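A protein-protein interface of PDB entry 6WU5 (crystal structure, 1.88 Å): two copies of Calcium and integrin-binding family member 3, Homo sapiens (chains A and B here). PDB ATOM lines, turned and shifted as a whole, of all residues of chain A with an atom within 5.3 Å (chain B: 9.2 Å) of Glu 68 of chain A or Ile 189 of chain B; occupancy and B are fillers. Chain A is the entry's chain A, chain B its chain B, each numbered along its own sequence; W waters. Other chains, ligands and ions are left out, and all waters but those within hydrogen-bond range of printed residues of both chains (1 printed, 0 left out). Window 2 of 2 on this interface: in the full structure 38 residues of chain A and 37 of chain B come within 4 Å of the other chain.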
ATOM      1  N   ARG A  37      -9.136 -13.128   1.229  1.00  0.00           N
ATOM      2  CA  ARG A  37      -7.840 -12.956   1.883  1.00  0.00           C
ATOM      3  C   ARG A  37      -6.734 -12.760   0.848  1.00  0.00           C
ATOM      4  O   ARG A  37      -5.871 -11.886   1.000  1.00  0.00           O
ATOM      5  CB  ARG A  37      -7.522 -14.169   2.764  1.00  0.00           C
ATOM      6  CG  ARG A  37      -8.387 -14.286   3.997  1.00  0.00           C
ATOM      7  CD  ARG A  37      -7.586 -14.691   5.236  1.00  0.00           C
ATOM      8  NE  ARG A  37      -6.323 -13.966   5.377  1.00  0.00           N
ATOM      9  CZ  ARG A  37      -5.358 -14.309   6.227  1.00  0.00           C
ATOM     10  NH1 ARG A  37      -5.518 -15.362   7.016  1.00  0.00           N
ATOM     11  NH2 ARG A  37      -4.237 -13.604   6.287  1.00  0.00           N
ATOM     12  N   MET A  66       2.419 -13.120   5.646  1.00  0.00           N
ATOM     13  CA  MET A  66       1.108 -13.439   6.186  1.00  0.00           C
ATOM     14  C   MET A  66       1.244 -13.994   7.604  1.00  0.00           C
ATOM     15  O   MET A  66       2.209 -14.699   7.909  1.00  0.00           O
ATOM     16  CB  MET A  66       0.405 -14.480   5.328  1.00  0.00           C
ATOM     17  CG  MET A  66      -0.008 -14.016   3.962  1.00  0.00           C
ATOM     18  SD  MET A  66      -0.714 -15.421   3.089  1.00  0.00           S
ATOM     19  CE  MET A  66      -2.292 -15.652   3.891  1.00  0.00           C
ATOM     20  N   PRO A  67       0.260 -13.737   8.473  1.00  0.00           N
ATOM     21  CA  PRO A  67       0.371 -14.237   9.855  1.00  0.00           C
ATOM     22  C   PRO A  67       0.526 -15.742   9.941  1.00  0.00           C
ATOM     23  O   PRO A  67       1.141 -16.241  10.894  1.00  0.00           O
ATOM     24  CB  PRO A  67      -0.935 -13.768  10.518  1.00  0.00           C
ATOM     25  CG  PRO A  67      -1.813 -13.248   9.410  1.00  0.00           C
ATOM     26  CD  PRO A  67      -0.919 -12.875   8.270  1.00  0.00           C
ATOM     27  N   GLU A  68      -0.013 -16.480   8.969  1.00  0.00           N
ATOM     28  CA  GLU A  68       0.081 -17.932   8.973  1.00  0.00           C
ATOM     29  C   GLU A  68       1.458 -18.445   8.581  1.00  0.00           C
ATOM     30  O   GLU A  68       1.746 -19.626   8.798  1.00  0.00           O
ATOM     31  CB  GLU A  68      -0.956 -18.516   8.010  1.00  0.00           C
ATOM     32  CG  GLU A  68      -2.391 -18.362   8.466  1.00  0.00           C
ATOM     33  CD  GLU A  68      -2.975 -16.991   8.167  1.00  0.00           C
ATOM     34  OE1 GLU A  68      -4.061 -16.693   8.702  1.00  0.00           O
ATOM     35  OE2 GLU A  68      -2.361 -16.213   7.408  1.00  0.00           O
ATOM     36  N   LEU A  69       2.302 -17.604   7.977  1.00  0.00           N
ATOM     37  CA  LEU A  69       3.626 -18.025   7.539  1.00  0.00           C
ATOM     38  C   LEU A  69       4.765 -17.218   8.139  1.00  0.00           C
ATOM     39  O   LEU A  69       5.909 -17.687   8.090  1.00  0.00           O
ATOM     40  CB  LEU A  69       3.739 -17.935   6.010  1.00  0.00           C
ATOM     41  CG  LEU A  69       2.861 -18.889   5.202  1.00  0.00           C
ATOM     42  CD1 LEU A  69       2.987 -18.544   3.717  1.00  0.00           C
ATOM     43  CD2 LEU A  69       3.225 -20.340   5.452  1.00  0.00           C
ATOM     44  N   LYS A  70       4.484 -16.037   8.709  1.00  0.00           N
ATOM     45  CA  LYS A  70       5.507 -15.166   9.277  1.00  0.00           C
ATOM     46  C   LYS A  70       6.522 -15.892  10.139  1.00  0.00           C
ATOM     47  O   LYS A  70       7.734 -15.667  10.027  1.00  0.00           O
ATOM     48  CB  LYS A  70       4.842 -14.084  10.143  1.00  0.00           C
ATOM     49  CG  LYS A  70       4.652 -12.750   9.480  1.00  0.00           C
ATOM     50  CD  LYS A  70       4.349 -11.675  10.510  1.00  0.00           C
ATOM     51  CE  LYS A  70       4.344 -10.284   9.888  1.00  0.00           C
ATOM     52  NZ  LYS A  70       4.873  -9.258  10.831  1.00  0.00           N
ATOM     53  N   ASN A  72       7.013 -19.148  10.455  1.00  0.00           N
ATOM     54  CA  ASN A  72       7.371 -20.475   9.973  1.00  0.00           C
ATOM     55  C   ASN A  72       8.807 -20.451   9.479  1.00  0.00           C
ATOM     56  O   ASN A  72       9.110 -19.695   8.546  1.00  0.00           O
ATOM     57  CB  ASN A  72       6.427 -20.897   8.861  1.00  0.00           C
ATOM     58  CG  ASN A  72       6.535 -22.366   8.528  1.00  0.00           C
ATOM     59  OD1 ASN A  72       7.632 -22.902   8.408  1.00  0.00           O
ATOM     60  ND2 ASN A  72       5.385 -23.023   8.361  1.00  0.00           N
ATOM     61  N   PHE A  99      -2.892 -23.627   1.342  1.00  0.00           N
ATOM     62  CA  PHE A  99      -3.689 -23.596   2.572  1.00  0.00           C
ATOM     63  C   PHE A  99      -4.555 -24.837   2.706  1.00  0.00           C
ATOM     64  O   PHE A  99      -4.862 -25.247   3.829  1.00  0.00           O
ATOM     65  CB  PHE A  99      -4.494 -22.316   2.623  1.00  0.00           C
ATOM     66  CG  PHE A  99      -3.664 -21.135   3.023  1.00  0.00           C
ATOM     67  CD1 PHE A  99      -3.073 -21.078   4.277  1.00  0.00           C
ATOM     68  CD2 PHE A  99      -3.413 -20.118   2.138  1.00  0.00           C
ATOM     69  CE1 PHE A  99      -2.280 -20.000   4.635  1.00  0.00           C
ATOM     70  CE2 PHE A  99      -2.638 -19.045   2.483  1.00  0.00           C
ATOM     71  CZ  PHE A  99      -2.061 -18.985   3.729  1.00  0.00           C
ATOM     72  N   MET A 102      -2.181 -27.144   4.350  1.00  0.00           N
ATOM     73  CA  MET A 102      -1.921 -26.700   5.717  1.00  0.00           C
ATOM     74  C   MET A 102      -3.154 -26.756   6.605  1.00  0.00           C
ATOM     75  O   MET A 102      -3.023 -26.609   7.825  1.00  0.00           O
ATOM     76  CB  MET A 102      -1.345 -25.280   5.683  1.00  0.00           C
ATOM     77  CG  MET A 102      -0.029 -25.223   4.920  1.00  0.00           C
ATOM     78  SD  MET A 102       0.889 -23.684   5.047  1.00  0.00           S
ATOM     79  CE  MET A 102       1.582 -23.881   6.692  1.00  0.00           C
ATOM     80  N   GLU A 104      -6.533 -28.013   8.755  1.00  0.00           N
ATOM     81  CA  GLU A 104      -6.768 -29.101   9.695  1.00  0.00           C
ATOM     82  C   GLU A 104      -7.410 -30.307   9.019  1.00  0.00           C
ATOM     83  O   GLU A 104      -7.374 -31.405   9.579  1.00  0.00           O
ATOM     84  CB  GLU A 104      -7.647 -28.612  10.847  1.00  0.00           C
ATOM     85  CG  GLU A 104      -6.896 -28.429  12.165  1.00  0.00           C
ATOM     86  CD  GLU A 104      -5.895 -27.283  12.121  1.00  0.00           C
ATOM     87  OE1 GLU A 104      -4.681 -27.538  12.292  1.00  0.00           O
ATOM     88  OE2 GLU A 104      -6.321 -26.128  11.919  1.00  0.00           O
ATOM     89  N   GLY B 142       0.081 -26.067  24.719  1.00  0.00           N
ATOM     90  CA  GLY B 142       0.000 -24.948  23.813  1.00  0.00           C
ATOM     91  C   GLY B 142       0.506 -25.215  22.417  1.00  0.00           C
ATOM     92  O   GLY B 142       0.257 -24.398  21.520  1.00  0.00           O
ATOM     93  N   GLU B 143       1.202 -26.328  22.197  1.00  0.00           N
ATOM     94  CA  GLU B 143       1.722 -26.701  20.888  1.00  0.00           C
ATOM     95  C   GLU B 143       0.833 -27.717  20.183  1.00  0.00           C
ATOM     96  O   GLU B 143       0.500 -27.535  19.010  1.00  0.00           O
ATOM     97  CB  GLU B 143       3.140 -27.264  21.027  1.00  0.00           C
ATOM     98  CG  GLU B 143       4.110 -26.328  21.725  1.00  0.00           C
ATOM     99  CD  GLU B 143       5.490 -26.935  21.909  1.00  0.00           C
ATOM    100  OE1 GLU B 143       5.635 -28.172  21.772  1.00  0.00           O
ATOM    101  OE2 GLU B 143       6.433 -26.169  22.198  1.00  0.00           O
ATOM    102  N   SER B 145      -2.861 -29.886  20.238  1.00  0.00           N
ATOM    103  CA  SER B 145      -4.183 -30.003  20.820  1.00  0.00           C
ATOM    104  C   SER B 145      -4.365 -31.387  21.440  1.00  0.00           C
ATOM    105  O   SER B 145      -3.590 -32.319  21.203  1.00  0.00           O
ATOM    106  CB  SER B 145      -5.260 -29.767  19.765  1.00  0.00           C
ATOM    107  OG  SER B 145      -5.357 -30.896  18.915  1.00  0.00           O
ATOM    108  N   GLU B 148      -4.391 -33.816  18.737  1.00  0.00           N
ATOM    109  CA  GLU B 148      -3.068 -34.094  18.186  1.00  0.00           C
ATOM    110  C   GLU B 148      -2.250 -34.955  19.136  1.00  0.00           C
ATOM    111  O   GLU B 148      -1.549 -35.880  18.707  1.00  0.00           O
ATOM    112  CB  GLU B 148      -2.328 -32.789  17.891  1.00  0.00           C
ATOM    113  CG  GLU B 148      -2.906 -32.000  16.735  1.00  0.00           C
ATOM    114  CD  GLU B 148      -2.306 -30.607  16.627  1.00  0.00           C
ATOM    115  OE1 GLU B 148      -2.360 -29.845  17.618  1.00  0.00           O
ATOM    116  OE2 GLU B 148      -1.781 -30.269  15.551  1.00  0.00           O
ATOM    117  N   LEU B 184       6.293 -31.962  11.354  1.00  0.00           N
ATOM    118  CA  LEU B 184       5.090 -31.501  10.681  1.00  0.00           C
ATOM    119  C   LEU B 184       4.540 -30.219  11.295  1.00  0.00           C
ATOM    120  O   LEU B 184       3.459 -29.768  10.910  1.00  0.00           O
ATOM    121  CB  LEU B 184       4.024 -32.596  10.686  1.00  0.00           C
ATOM    122  CG  LEU B 184       4.410 -33.937  10.044  1.00  0.00           C
ATOM    123  CD1 LEU B 184       3.237 -34.916  10.087  1.00  0.00           C
ATOM    124  CD2 LEU B 184       4.900 -33.777   8.619  1.00  0.00           C
ATOM    125  N   SER B 185       5.274 -29.605  12.222  1.00  0.00           N
ATOM    126  CA  SER B 185       4.837 -28.326  12.766  1.00  0.00           C
ATOM    127  C   SER B 185       4.738 -27.278  11.668  1.00  0.00           C
ATOM    128  O   SER B 185       3.948 -26.332  11.780  1.00  0.00           O
ATOM    129  CB  SER B 185       5.797 -27.851  13.854  1.00  0.00           C
ATOM    130  OG  SER B 185       7.090 -27.629  13.325  1.00  0.00           O
ATOM    131  N   THR B 186       5.519 -27.440  10.599  1.00  0.00           N
ATOM    132  CA  THR B 186       5.534 -26.478   9.503  1.00  0.00           C
ATOM    133  C   THR B 186       4.266 -26.497   8.670  1.00  0.00           C
ATOM    134  O   THR B 186       4.094 -25.615   7.819  1.00  0.00           O
ATOM    135  CB  THR B 186       6.727 -26.756   8.584  1.00  0.00           C
ATOM    136  OG1 THR B 186       6.867 -28.171   8.409  1.00  0.00           O
ATOM    137  CG2 THR B 186       8.004 -26.191   9.173  1.00  0.00           C
ATOM    138  N   PHE B 187       3.388 -27.487   8.878  1.00  0.00           N
ATOM    139  CA  PHE B 187       2.174 -27.644   8.080  1.00  0.00           C
ATOM    140  C   PHE B 187       0.920 -27.686   8.940  1.00  0.00           C
ATOM    141  O   PHE B 187      -0.132 -28.130   8.474  1.00  0.00           O
ATOM    142  CB  PHE B 187       2.280 -28.901   7.221  1.00  0.00           C
ATOM    143  CG  PHE B 187       3.100 -28.699   5.996  1.00  0.00           C
ATOM    144  CD1 PHE B 187       2.530 -28.189   4.843  1.00  0.00           C
ATOM    145  CD2 PHE B 187       4.451 -28.971   6.007  1.00  0.00           C
ATOM    146  CE1 PHE B 187       3.295 -27.981   3.726  1.00  0.00           C
ATOM    147  CE2 PHE B 187       5.215 -28.762   4.886  1.00  0.00           C
ATOM    148  CZ  PHE B 187       4.645 -28.265   3.754  1.00  0.00           C
ATOM    149  N   HIS B 188       1.027 -27.250  10.195  1.00  0.00           N
ATOM    150  CA  HIS B 188      -0.098 -27.022  11.092  1.00  0.00           C
ATOM    151  C   HIS B 188      -0.027 -25.571  11.547  1.00  0.00           C
ATOM    152  O   HIS B 188       1.021 -25.126  12.029  1.00  0.00           O
ATOM    153  CB  HIS B 188      -0.057 -27.944  12.316  1.00  0.00           C
ATOM    154  CG  HIS B 188      -0.368 -29.376  12.009  1.00  0.00           C
ATOM    155  ND1 HIS B 188      -1.626 -29.915  12.169  1.00  0.00           N
ATOM    156  CD2 HIS B 188       0.420 -30.383  11.568  1.00  0.00           C
ATOM    157  CE1 HIS B 188      -1.603 -31.190  11.826  1.00  0.00           C
ATOM    158  NE2 HIS B 188      -0.374 -31.499  11.452  1.00  0.00           N
ATOM    159  N   ILE B 189      -1.126 -24.847  11.423  1.00  0.00           N
ATOM    160  CA  ILE B 189      -1.120 -23.402  11.625  1.00  0.00           C
ATOM    161  C   ILE B 189      -1.504 -23.072  13.061  1.00  0.00           C
ATOM    162  O   ILE B 189      -2.442 -23.653  13.618  1.00  0.00           O
ATOM    163  CB  ILE B 189      -2.075 -22.715  10.629  1.00  0.00           C
ATOM    164  CG1 ILE B 189      -1.606 -22.973   9.194  1.00  0.00           C
ATOM    165  CG2 ILE B 189      -2.170 -21.217  10.912  1.00  0.00           C
ATOM    166  CD1 ILE B 189      -2.523 -22.381   8.125  1.00  0.00           C
ATOM    167  N   ARG B 190      -0.786 -22.117  13.655  1.00  0.00           N
ATOM    168  CA  ARG B 190      -1.088 -21.638  15.003  1.00  0.00           C
ATOM    169  C   ARG B 190      -1.752 -20.265  14.958  1.00  0.00           C
ATOM    170  O   ARG B 190      -2.857 -20.080  15.464  1.00  0.00           O
ATOM    171  CB  ARG B 190       0.184 -21.568  15.853  1.00  0.00           C
HETATM  172  O   HOH W   1      -3.594 -26.211  10.349  1.00  0.00           O
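CG of Glu 68 of chain A touches CG2 of Ile 189 of chain B, 3.8 Å away.
Met 102 of chain A touches Thr 186 of chain B.
Met 102 of chain A touches Ile 189 of chain B (CB to CD1, 3.97 Å).
ND1 of His 188 of chain B touches OE1 of Glu 104 of chain A (3.9 Å).
Of the 11 printed residues of chain B, 4 touch a printed residue of chain A.
Hydrophobic or aromatic side chains of chain B within 4 Å of the printed part of chain A: Phe 187, His 188 and Ile 189.
Hydrophobic or aromatic side chains of chain A that line the printed part of chain B: Met 102.
Along chain A the printed residues that touch a printed residue of chain B span positions 68 to 104.
Among the printed residues, no Asp or Glu carboxylate lies within 4 Å of a Lys or Arg side-chain nitrogen of the other chain.
Of the printed residues of chain B, Glu 68 of chain A touches Ile 189.
Of chain A, only Glu 68 and Met 102 come within 4 Å of Ile 189 of chain B.
No residue of chain B comes within 4 Å of Leu 69 of chain A.
Of the printed residues of chain B, Glu 104 of chain A touches His 188 (3.9 Å).
Of the printed residues of chain A, Thr 186 of chain B touches Asn 72 (2.9 Å) and Met 102 (3.3 Å).
Gly 142 of chain B touches none of the printed residues of chain A.
The nearest residue of chain B that does not touch Glu 68 of chain A is Arg 190 of chain B (6.0 Å).
The nearest residue of chain A that does not touch Ile 189 of chain B is Phe 99 of chain A (4.1 Å).
The nearest printed residue of chain A that does not touch His 188 of chain B is Met 102 of chain A (4.4 Å).
Water W1 lies within hydrogen-bond range of OE1 of Glu 104 of chain A (2.6 Å), O of Met 102 of chain A (2.6 Å) and N of Ile 189 of chain B (3.0 Å).
No position is printed for both chains.
Of the 6 pairs that touch across the chains among the printed residues, none has its exchanged pair printed and touching as well.
The side-chain carboxylate of Glu 148 of chain B lies within hydrogen-bond range of a ring nitrogen (ND1) of His 188 of chain B (3.4 Å).
OE1 of Glu 68 of chain A is in salt-bridge range of NH1 of Arg 37 of chain A, 2.6 Å away.
O of Met 102 of chain A lies close to O of Phe 187 of chain B, 3.3 Å away.
The backbone carbonyl oxygen (O) of Thr 186 of chain B is in hydrogen-bond range of the side-chain amide nitrogen (ND2) of Asn 72 of chain A (2.9 Å).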
